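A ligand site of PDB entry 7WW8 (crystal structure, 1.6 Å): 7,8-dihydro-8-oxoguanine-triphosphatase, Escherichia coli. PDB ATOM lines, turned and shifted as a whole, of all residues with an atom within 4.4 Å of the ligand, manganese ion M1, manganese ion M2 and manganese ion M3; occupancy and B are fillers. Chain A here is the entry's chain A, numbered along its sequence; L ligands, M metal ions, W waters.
O9 of the ligand is in salt-bridge range of NH2 of Arg 23 (2.9 Å). An oxygen (O12) of the ligand is in hydrogen-bond range of a ring nitrogen (ND1) of His 28. OD1 of Asn 119 lies within hydrogen-bond range of N2 of the ligand (2.7 Å). The backbone carbonyl oxygen (O) of Phe 35 is in hydrogen-bond range of a nitrogen (N3) of the ligand (2.7 Å). An oxygen (O5) of the ligand lies close to the backbone NH of Lys 39, 2.9 Å away. The backbone NH (N) of Phe 35 lies within hydrogen-bond range of an oxygen (O13) of the ligand, at 3.0 Å. The side-chain carboxylate (OE1) of Glu 34 sits at hydrogen-bond distance from a nitrogen (N4) of the ligand.
The backbone carbonyl oxygen (O) of Lys 39 is in hydrogen-bond range of the guanidinium group (NH2) of Arg 52. The side-chain carboxylate (OE1) of Glu 34 is in salt-bridge range of the guanidinium group (NH1) of Arg 23 (2.9 Å). O of His 28 lies within hydrogen-bond range of NE of Arg 23, at 2.8 Å. NH1 of Arg 52 lies close to OE2 of Glu 53 (3.0 Å).
Merely in contact with the ligand: Pro 116 (3.3 Å), Phe 75 (3.3 Å), Gly 38 (3.4 Å), Ile 80 (3.4 Å), Val 8 (3.5 Å), Ala 118 (3.6 Å), Ile 6 (3.7 Å) and Leu 82 (3.7 Å). The nearest printed residue that does not touch the ligand is Arg 78 (4.2 Å).
Gly 38 touches manganese ion M1. Of the 23 residues printed, 3 come within 4 Å of manganese ion M1. The nearest printed residue that does not touch manganese ion M1 is Arg 23 (4.2 Å).
One residue has an atom within 4 Å of manganese ion M2: Glu 53. The nearest printed residue that does not touch manganese ion M2 is Lys 39 (4.1 Å).
Within 4 Å of manganese ion M3: Gly 37, Glu 53 and Glu 57.
O of Gly 37 binds manganese ion M1, 2.1 Å away. Manganese ion M1 is bound by an oxygen (O6) of the ligand. Manganese ion M1 is bound by O8 of the ligand, at 2.2 Å. Water W10 is bound to manganese ion M1, at 2.2 Å. Manganese ion M1 is bound by OE2 of Glu 57 (2.2 Å). Water W2 binds manganese ion M1 (2.2 Å). Manganese ion M1 has six donor atoms within binding distance.
Manganese ion M2 is bound by water W1 (2.3 Å), water W7 (2.3 Å), water W8 (2.3 Å), water W3 (2.3 Å), O5 of the ligand (2.4 Å) and OE2 of Glu 53 (2.4 Å).
OE2 of Glu 57 is bound to manganese ion M3 (2.3 Å). O6 of the ligand binds manganese ion M3 (2.3 Å). Water W1 is bound to manganese ion M3 (2.3 Å). Manganese ion M3 is bound by water W6 (2.3 Å). Water W4 is bound to manganese ion M3 (2.3 Å). Manganese ion M3 is bound by OE1 of Glu 53, at 2.4 Å.
Water W10 lies within hydrogen-bond range of the side-chain carboxylate (OE1) of Glu 34, the side-chain carboxylate (OE1) of Glu 57 and a nitrogen (N4) of the ligand. Water W3 bridges OE1 of Glu 56 (2.7 Å) and NH1 of Arg 52 (3.2 Å). Water W8 lies within hydrogen-bond range of the backbone carbonyl oxygen of Lys 39 (2.8 Å) and the guanidinium group of Arg 52 (3.5 Å). Water W6 bridges OE2 of Glu 98 and OE1 of Glu 56. Water W4 bridges O1 of the ligand and OE1 of Glu 98. Water W9 lies within hydrogen-bond range of the guanidinium group (NH1) of Arg 78 and an oxygen (O12) of the ligand.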
ATOM      1  N   ILE A   6     -15.727  33.615 -23.358  1.00  0.00           N
ATOM      2  CA  ILE A   6     -16.583  33.122 -24.447  1.00  0.00           C
ATOM      3  C   ILE A   6     -17.096  34.317 -25.238  1.00  0.00           C
ATOM      4  O   ILE A   6     -17.603  35.272 -24.646  1.00  0.00           O
ATOM      5  CB  ILE A   6     -17.751  32.294 -23.903  1.00  0.00           C
ATOM      6  CG1 ILE A   6     -17.289  31.155 -22.979  1.00  0.00           C
ATOM      7  CG2 ILE A   6     -18.637  31.780 -25.045  1.00  0.00           C
ATOM      8  CD1 ILE A   6     -16.332  30.163 -23.611  1.00  0.00           C
ATOM      9  N   VAL A   8     -19.870  35.315 -28.230  1.00  0.00           N
ATOM     10  CA  VAL A   8     -21.024  34.827 -28.962  1.00  0.00           C
ATOM     11  C   VAL A   8     -21.635  35.957 -29.780  1.00  0.00           C
ATOM     12  O   VAL A   8     -21.439  37.148 -29.497  1.00  0.00           O
ATOM     13  CB  VAL A   8     -22.100  34.198 -28.037  1.00  0.00           C
ATOM     14  CG1 VAL A   8     -21.463  33.220 -27.065  1.00  0.00           C
ATOM     15  CG2 VAL A   8     -22.858  35.284 -27.284  1.00  0.00           C
ATOM     16  N   ARG A  23     -27.496  23.225 -28.572  1.00  0.00           N
ATOM     17  CA  ARG A  23     -26.273  22.568 -28.159  1.00  0.00           C
ATOM     18  C   ARG A  23     -26.439  21.053 -28.085  1.00  0.00           C
ATOM     19  O   ARG A  23     -27.526  20.542 -27.781  1.00  0.00           O
ATOM     20  CB  ARG A  23     -25.789  23.113 -26.816  1.00  0.00           C
ATOM     21  CG  ARG A  23     -25.439  24.580 -26.910  1.00  0.00           C
ATOM     22  CD  ARG A  23     -24.966  25.162 -25.590  1.00  0.00           C
ATOM     23  NE  ARG A  23     -23.753  24.522 -25.065  1.00  0.00           N
ATOM     24  CZ  ARG A  23     -22.519  24.818 -25.465  1.00  0.00           C
ATOM     25  NH1 ARG A  23     -22.308  25.718 -26.429  1.00  0.00           N
ATOM     26  NH2 ARG A  23     -21.491  24.178 -24.909  1.00  0.00           N
ATOM     27  N   HIS A  28     -21.423  20.812 -22.381  1.00  0.00           N
ATOM     28  CA  HIS A  28     -21.851  21.672 -21.290  1.00  0.00           C
ATOM     29  C   HIS A  28     -23.074  22.456 -21.754  1.00  0.00           C
ATOM     30  O   HIS A  28     -23.157  22.864 -22.913  1.00  0.00           O
ATOM     31  CB  HIS A  28     -20.720  22.626 -20.868  1.00  0.00           C
ATOM     32  CG  HIS A  28     -21.061  23.457 -19.684  1.00  0.00           C
ATOM     33  ND1 HIS A  28     -21.260  24.825 -19.749  1.00  0.00           N
ATOM     34  CD2 HIS A  28     -21.271  23.119 -18.385  1.00  0.00           C
ATOM     35  CE1 HIS A  28     -21.569  25.282 -18.552  1.00  0.00           C
ATOM     36  NE2 HIS A  28     -21.586  24.269 -17.710  1.00  0.00           N
ATOM     37  N   MET A  29     -24.046  22.633 -20.855  1.00  0.00           N
ATOM     38  CA  MET A  29     -25.338  23.245 -21.192  1.00  0.00           C
ATOM     39  C   MET A  29     -25.989  22.463 -22.333  1.00  0.00           C
ATOM     40  O   MET A  29     -26.450  23.025 -23.328  1.00  0.00           O
ATOM     41  CB  MET A  29     -25.180  24.732 -21.535  1.00  0.00           C
ATOM     42  CG  MET A  29     -24.943  25.611 -20.310  1.00  0.00           C
ATOM     43  SD  MET A  29     -26.353  25.569 -19.160  1.00  0.00           S
ATOM     44  CE  MET A  29     -25.725  24.542 -17.814  1.00  0.00           C
ATOM     45  N   GLU A  34     -28.889  28.521 -27.922  1.00  0.00           N
ATOM     46  CA  GLU A  34     -27.681  29.296 -27.714  1.00  0.00           C
ATOM     47  C   GLU A  34     -27.488  30.284 -28.843  1.00  0.00           C
ATOM     48  O   GLU A  34     -27.944  30.071 -29.964  1.00  0.00           O
ATOM     49  CB  GLU A  34     -26.451  28.381 -27.641  1.00  0.00           C
ATOM     50  CG  GLU A  34     -26.336  27.546 -28.901  1.00  0.00           C
ATOM     51  CD  GLU A  34     -24.969  26.924 -29.136  1.00  0.00           C
ATOM     52  OE1 GLU A  34     -24.053  27.126 -28.307  1.00  0.00           O
ATOM     53  OE2 GLU A  34     -24.839  26.226 -30.167  1.00  0.00           O
ATOM     54  N   PHE A  35     -26.784  31.381 -28.536  1.00  0.00           N
ATOM     55  CA  PHE A  35     -26.188  32.187 -29.591  1.00  0.00           C
ATOM     56  C   PHE A  35     -24.909  31.509 -30.073  1.00  0.00           C
ATOM     57  O   PHE A  35     -24.114  31.075 -29.242  1.00  0.00           O
ATOM     58  CB  PHE A  35     -25.866  33.597 -29.062  1.00  0.00           C
ATOM     59  CG  PHE A  35     -27.039  34.293 -28.447  1.00  0.00           C
ATOM     60  CD1 PHE A  35     -28.164  34.581 -29.205  1.00  0.00           C
ATOM     61  CD2 PHE A  35     -27.007  34.709 -27.128  1.00  0.00           C
ATOM     62  CE1 PHE A  35     -29.257  35.235 -28.646  1.00  0.00           C
ATOM     63  CE2 PHE A  35     -28.082  35.365 -26.556  1.00  0.00           C
ATOM     64  CZ  PHE A  35     -29.219  35.632 -27.316  1.00  0.00           C
ATOM     65  N   PRO A  36     -24.686  31.381 -31.374  1.00  0.00           N
ATOM     66  CA  PRO A  36     -23.424  30.759 -31.825  1.00  0.00           C
ATOM     67  C   PRO A  36     -22.224  31.496 -31.253  1.00  0.00           C
ATOM     68  O   PRO A  36     -22.231  32.724 -31.107  1.00  0.00           O
ATOM     69  CB  PRO A  36     -23.495  30.882 -33.355  1.00  0.00           C
ATOM     70  CG  PRO A  36     -24.981  30.917 -33.637  1.00  0.00           C
ATOM     71  CD  PRO A  36     -25.548  31.747 -32.515  1.00  0.00           C
ATOM     72  N   GLY A  37     -21.187  30.742 -30.903  1.00  0.00           N
ATOM     73  CA  GLY A  37     -19.994  31.347 -30.336  1.00  0.00           C
ATOM     74  C   GLY A  37     -19.129  30.290 -29.668  1.00  0.00           C
ATOM     75  O   GLY A  37     -19.404  29.102 -29.740  1.00  0.00           O
ATOM     76  N   GLY A  38     -18.069  30.758 -29.010  1.00  0.00           N
ATOM     77  CA  GLY A  38     -17.186  29.823 -28.356  1.00  0.00           C
ATOM     78  C   GLY A  38     -16.020  30.494 -27.688  1.00  0.00           C
ATOM     79  O   GLY A  38     -16.010  31.710 -27.481  1.00  0.00           O
ATOM     80  N   LYS A  39     -15.019  29.673 -27.358  1.00  0.00           N
ATOM     81  CA  LYS A  39     -13.928  30.118 -26.507  1.00  0.00           C
ATOM     82  C   LYS A  39     -12.981  31.062 -27.227  1.00  0.00           C
ATOM     83  O   LYS A  39     -12.560  30.799 -28.361  1.00  0.00           O
ATOM     84  CB  LYS A  39     -13.164  28.893 -25.987  1.00  0.00           C
ATOM     85  CG  LYS A  39     -14.047  27.935 -25.199  1.00  0.00           C
ATOM     86  CD  LYS A  39     -13.514  26.508 -25.124  1.00  0.00           C
ATOM     87  CE  LYS A  39     -14.536  25.604 -24.434  1.00  0.00           C
ATOM     88  NZ  LYS A  39     -14.024  24.236 -24.140  1.00  0.00           N
ATOM     89  N   ARG A  52     -14.346  34.492 -35.872  1.00  0.00           N
ATOM     90  CA  ARG A  52     -13.897  33.128 -36.144  1.00  0.00           C
ATOM     91  C   ARG A  52     -14.963  32.098 -35.765  1.00  0.00           C
ATOM     92  O   ARG A  52     -15.242  31.166 -36.528  1.00  0.00           O
ATOM     93  CB  ARG A  52     -12.598  32.839 -35.388  1.00  0.00           C
ATOM     94  CG  ARG A  52     -12.085  31.418 -35.619  1.00  0.00           C
ATOM     95  CD  ARG A  52     -10.850  31.095 -34.753  1.00  0.00           C
ATOM     96  NE  ARG A  52     -11.071  31.446 -33.358  1.00  0.00           N
ATOM     97  CZ  ARG A  52     -11.860  30.750 -32.537  1.00  0.00           C
ATOM     98  NH1 ARG A  52     -12.484  29.656 -32.975  1.00  0.00           N
ATOM     99  NH2 ARG A  52     -12.036  31.152 -31.285  1.00  0.00           N
ATOM    100  N   GLU A  53     -15.557  32.249 -34.575  1.00  0.00           N
ATOM    101  CA  GLU A  53     -16.530  31.267 -34.114  1.00  0.00           C
ATOM    102  C   GLU A  53     -17.768  31.243 -35.009  1.00  0.00           C
ATOM    103  O   GLU A  53     -18.338  30.176 -35.273  1.00  0.00           O
ATOM    104  CB  GLU A  53     -16.919  31.535 -32.662  1.00  0.00           C
ATOM    105  CG  GLU A  53     -15.827  31.151 -31.664  1.00  0.00           C
ATOM    106  CD  GLU A  53     -15.715  29.659 -31.483  1.00  0.00           C
ATOM    107  OE1 GLU A  53     -16.670  28.926 -31.812  1.00  0.00           O
ATOM    108  OE2 GLU A  53     -14.663  29.199 -30.982  1.00  0.00           O
ATOM    109  N   GLU A  56     -16.864  29.426 -38.179  1.00  0.00           N
ATOM    110  CA  GLU A  56     -16.780  27.984 -37.965  1.00  0.00           C
ATOM    111  C   GLU A  56     -18.162  27.374 -37.766  1.00  0.00           C
ATOM    112  O   GLU A  56     -18.487  26.316 -38.332  1.00  0.00           O
ATOM    113  CB  GLU A  56     -15.916  27.673 -36.742  1.00  0.00           C
ATOM    114  CG  GLU A  56     -14.454  28.017 -36.873  1.00  0.00           C
ATOM    115  CD  GLU A  56     -13.682  27.755 -35.588  1.00  0.00           C
ATOM    116  OE1 GLU A  56     -14.278  27.216 -34.630  1.00  0.00           O
ATOM    117  OE2 GLU A  56     -12.478  28.091 -35.540  1.00  0.00           O
ATOM    118  N   GLU A  57     -18.976  27.993 -36.913  1.00  0.00           N
ATOM    119  CA  GLU A  57     -20.195  27.330 -36.471  1.00  0.00           C
ATOM    120  C   GLU A  57     -21.334  27.496 -37.455  1.00  0.00           C
ATOM    121  O   GLU A  57     -22.139  26.567 -37.632  1.00  0.00           O
ATOM    122  CB  GLU A  57     -20.611  27.840 -35.082  1.00  0.00           C
ATOM    123  CG  GLU A  57     -19.646  27.396 -34.004  1.00  0.00           C
ATOM    124  CD  GLU A  57     -20.204  27.444 -32.601  1.00  0.00           C
ATOM    125  OE1 GLU A  57     -21.325  27.969 -32.419  1.00  0.00           O
ATOM    126  OE2 GLU A  57     -19.513  26.942 -31.688  1.00  0.00           O
ATOM    127  N   PHE A  75     -21.176  28.866 -13.183  1.00  0.00           N
ATOM    128  CA  PHE A  75     -21.816  27.577 -13.322  1.00  0.00           C
ATOM    129  C   PHE A  75     -21.345  26.651 -12.201  1.00  0.00           C
ATOM    130  O   PHE A  75     -20.383  26.974 -11.480  1.00  0.00           O
ATOM    131  CB  PHE A  75     -21.481  26.964 -14.687  1.00  0.00           C
ATOM    132  CG  PHE A  75     -22.197  27.624 -15.825  1.00  0.00           C
ATOM    133  CD1 PHE A  75     -23.524  27.310 -16.108  1.00  0.00           C
ATOM    134  CD2 PHE A  75     -21.528  28.521 -16.647  1.00  0.00           C
ATOM    135  CE1 PHE A  75     -24.182  27.913 -17.183  1.00  0.00           C
ATOM    136  CE2 PHE A  75     -22.174  29.108 -17.718  1.00  0.00           C
ATOM    137  CZ  PHE A  75     -23.501  28.811 -17.984  1.00  0.00           C
ATOM    138  N   ARG A  78     -17.691  25.657 -13.492  1.00  0.00           N
ATOM    139  CA  ARG A  78     -16.826  26.513 -14.286  1.00  0.00           C
ATOM    140  C   ARG A  78     -17.312  27.948 -14.196  1.00  0.00           C
ATOM    141  O   ARG A  78     -18.509  28.209 -13.997  1.00  0.00           O
ATOM    142  CB  ARG A  78     -16.774  26.051 -15.748  1.00  0.00           C
ATOM    143  CG  ARG A  78     -18.068  26.204 -16.516  1.00  0.00           C
ATOM    144  CD  ARG A  78     -17.987  25.391 -17.796  1.00  0.00           C
ATOM    145  NE  ARG A  78     -18.029  23.969 -17.476  1.00  0.00           N
ATOM    146  CZ  ARG A  78     -17.680  22.985 -18.306  1.00  0.00           C
ATOM    147  NH1 ARG A  78     -17.239  23.257 -19.520  1.00  0.00           N
ATOM    148  NH2 ARG A  78     -17.766  21.727 -17.893  1.00  0.00           N
ATOM    149  N   ILE A  80     -17.438  31.500 -16.316  1.00  0.00           N
ATOM    150  CA  ILE A  80     -17.297  31.985 -17.684  1.00  0.00           C
ATOM    151  C   ILE A  80     -17.628  33.472 -17.746  1.00  0.00           C
ATOM    152  O   ILE A  80     -18.483  33.972 -17.010  1.00  0.00           O
ATOM    153  CB  ILE A  80     -18.138  31.195 -18.698  1.00  0.00           C
ATOM    154  CG1 ILE A  80     -19.601  31.605 -18.661  1.00  0.00           C
ATOM    155  CG2 ILE A  80     -17.991  29.685 -18.484  1.00  0.00           C
ATOM    156  CD1 ILE A  80     -20.349  31.061 -19.826  1.00  0.00           C
ATOM    157  N   LEU A  82     -18.894  36.046 -20.594  1.00  0.00           N
ATOM    158  CA  LEU A  82     -19.570  35.999 -21.890  1.00  0.00           C
ATOM    159  C   LEU A  82     -19.578  37.378 -22.525  1.00  0.00           C
ATOM    160  O   LEU A  82     -20.021  38.347 -21.908  1.00  0.00           O
ATOM    161  CB  LEU A  82     -20.999  35.505 -21.753  1.00  0.00           C
ATOM    162  CG  LEU A  82     -21.153  34.000 -21.617  1.00  0.00           C
ATOM    163  CD1 LEU A  82     -22.371  33.742 -20.761  1.00  0.00           C
ATOM    164  CD2 LEU A  82     -21.292  33.311 -22.981  1.00  0.00           C
ATOM    165  N   GLU A  98     -21.718  23.011 -38.569  1.00  0.00           N
ATOM    166  CA  GLU A  98     -21.141  21.919 -37.802  1.00  0.00           C
ATOM    167  C   GLU A  98     -22.140  20.782 -37.559  1.00  0.00           C
ATOM    168  O   GLU A  98     -21.936  19.968 -36.649  1.00  0.00           O
ATOM    169  CB  GLU A  98     -20.571  22.447 -36.478  1.00  0.00           C
ATOM    170  CG  GLU A  98     -19.314  23.316 -36.677  1.00  0.00           C
ATOM    171  CD  GLU A  98     -18.720  23.832 -35.365  1.00  0.00           C
ATOM    172  OE1 GLU A  98     -19.415  23.801 -34.328  1.00  0.00           O
ATOM    173  OE2 GLU A  98     -17.557  24.299 -35.384  1.00  0.00           O
ATOM    174  N   PRO A 116     -29.014  28.850 -21.640  1.00  0.00           N
ATOM    175  CA  PRO A 116     -28.281  28.804 -20.383  1.00  0.00           C
ATOM    176  C   PRO A 116     -28.686  29.972 -19.500  1.00  0.00           C
ATOM    177  O   PRO A 116     -29.035  31.051 -19.991  1.00  0.00           O
ATOM    178  CB  PRO A 116     -26.812  28.923 -20.818  1.00  0.00           C
ATOM    179  CG  PRO A 116     -26.823  28.395 -22.257  1.00  0.00           C
ATOM    180  CD  PRO A 116     -28.112  28.925 -22.807  1.00  0.00           C
ATOM    181  N   ALA A 118     -27.079  31.997 -17.813  1.00  0.00           N
ATOM    182  CA  ALA A 118     -26.258  33.183 -17.993  1.00  0.00           C
ATOM    183  C   ALA A 118     -26.872  34.164 -18.973  1.00  0.00           C
ATOM    184  O   ALA A 118     -26.574  35.367 -18.904  1.00  0.00           O
ATOM    185  CB  ALA A 118     -24.863  32.777 -18.473  1.00  0.00           C
ATOM    186  N   ASN A 119     -27.727  33.698 -19.887  1.00  0.00           N
ATOM    187  CA  ASN A 119     -28.273  34.550 -20.933  1.00  0.00           C
ATOM    188  C   ASN A 119     -29.482  35.358 -20.488  1.00  0.00           C
ATOM    189  O   ASN A 119     -29.962  36.189 -21.276  1.00  0.00           O
ATOM    190  CB  ASN A 119     -28.672  33.707 -22.150  1.00  0.00           C
ATOM    191  CG  ASN A 119     -27.476  33.107 -22.859  1.00  0.00           C
ATOM    192  OD1 ASN A 119     -26.427  32.877 -22.267  1.00  0.00           O
ATOM    193  ND2 ASN A 119     -27.646  32.824 -24.149  1.00  0.00           N
HETATM  194  P1  LIG L   1     -16.108  23.375 -29.071  1.00  0.00           P
HETATM  195  O1  LIG L   1     -17.202  23.501 -30.096  1.00  0.00           O
HETATM  196  O2  LIG L   1     -16.270  22.149 -28.207  1.00  0.00           O
HETATM  197  O3  LIG L   1     -14.702  23.555 -29.585  1.00  0.00           O
HETATM  198  O4  LIG L   1     -16.315  24.595 -28.028  1.00  0.00           O
HETATM  199  P2  LIG L   1     -16.624  26.153 -28.346  1.00  0.00           P
HETATM  200  O5  LIG L   1     -15.387  26.996 -28.314  1.00  0.00           O
HETATM  201  O6  LIG L   1     -17.643  26.367 -29.444  1.00  0.00           O
HETATM  202  O7  LIG L   1     -17.202  26.617 -26.923  1.00  0.00           O
HETATM  203  P3  LIG L   1     -18.706  26.439 -26.416  1.00  0.00           P
HETATM  204  O8  LIG L   1     -19.662  27.135 -27.349  1.00  0.00           O
HETATM  205  O9  LIG L   1     -18.966  25.014 -26.028  1.00  0.00           O
HETATM  206  O10 LIG L   1     -18.542  27.318 -25.067  1.00  0.00           O
HETATM  207  C1  LIG L   1     -19.612  28.142 -24.657  1.00  0.00           C
HETATM  208  C2  LIG L   1     -19.662  28.133 -23.130  1.00  0.00           C
HETATM  209  O11 LIG L   1     -20.424  29.249 -22.740  1.00  0.00           O
HETATM  210  C3  LIG L   1     -20.411  26.924 -22.612  1.00  0.00           C
HETATM  211  O12 LIG L   1     -20.007  26.702 -21.253  1.00  0.00           O
HETATM  212  C4  LIG L   1     -21.851  27.391 -22.617  1.00  0.00           C
HETATM  213  C5  LIG L   1     -21.687  28.855 -22.237  1.00  0.00           C
HETATM  214  N1  LIG L   1     -22.766  29.660 -22.845  1.00  0.00           N
HETATM  215  C6  LIG L   1     -23.714  30.343 -22.222  1.00  0.00           C
HETATM  216  N2  LIG L   1     -24.565  31.005 -23.025  1.00  0.00           N
HETATM  217  C7  LIG L   1     -24.088  30.712 -24.255  1.00  0.00           C
HETATM  218  C8  LIG L   1     -24.508  31.097 -25.615  1.00  0.00           C
HETATM  219  O13 LIG L   1     -25.515  31.809 -25.804  1.00  0.00           O
HETATM  220  N3  LIG L   1     -23.781  30.628 -26.640  1.00  0.00           N
HETATM  221  C9  LIG L   1     -22.700  29.830 -26.461  1.00  0.00           C
HETATM  222  N4  LIG L   1     -21.997  29.407 -27.540  1.00  0.00           N
HETATM  223  N5  LIG L   1     -22.281  29.464 -25.236  1.00  0.00           N
HETATM  224  C10 LIG L   1     -22.967  29.890 -24.143  1.00  0.00           C
HETATM  225  O14 LIG L   1     -23.823  30.350 -20.938  1.00  0.00           O
HETATM  226 MN    MN M   1     -19.694  26.997 -29.501  1.00  0.00          MN
HETATM  227 MN    MN M   2     -14.008  26.989 -30.264  1.00  0.00          MN
HETATM  228 MN    MN M   3     -17.281  26.589 -31.697  1.00  0.00          MN
HETATM  229  O   HOH W   1     -15.419  25.384 -31.085  1.00  0.00           O
HETATM  230  O   HOH W   2     -20.339  24.867 -29.527  1.00  0.00           O
HETATM  231  O   HOH W   3     -12.962  26.586 -32.309  1.00  0.00           O
HETATM  232  O   HOH W   4     -18.131  24.466 -32.100  1.00  0.00           O
HETATM  233  O   HOH W   5     -17.907  23.934 -23.608  1.00  0.00           O
HETATM  234  O   HOH W   6     -16.501  26.078 -33.815  1.00  0.00           O
HETATM  235  O   HOH W   7     -12.835  25.063 -29.835  1.00  0.00           O
HETATM  236  O   HOH W   8     -12.219  28.225 -29.458  1.00  0.00           O
HETATM  237  O   HOH W   9     -17.477  25.422 -21.335  1.00  0.00           O
HETATM  238  O   HOH W  10     -21.818  27.475 -29.783  1.00  0.00           O
HETATM  239  O   HOH W  11     -19.099  22.868 -27.493  1.00  0.00           O
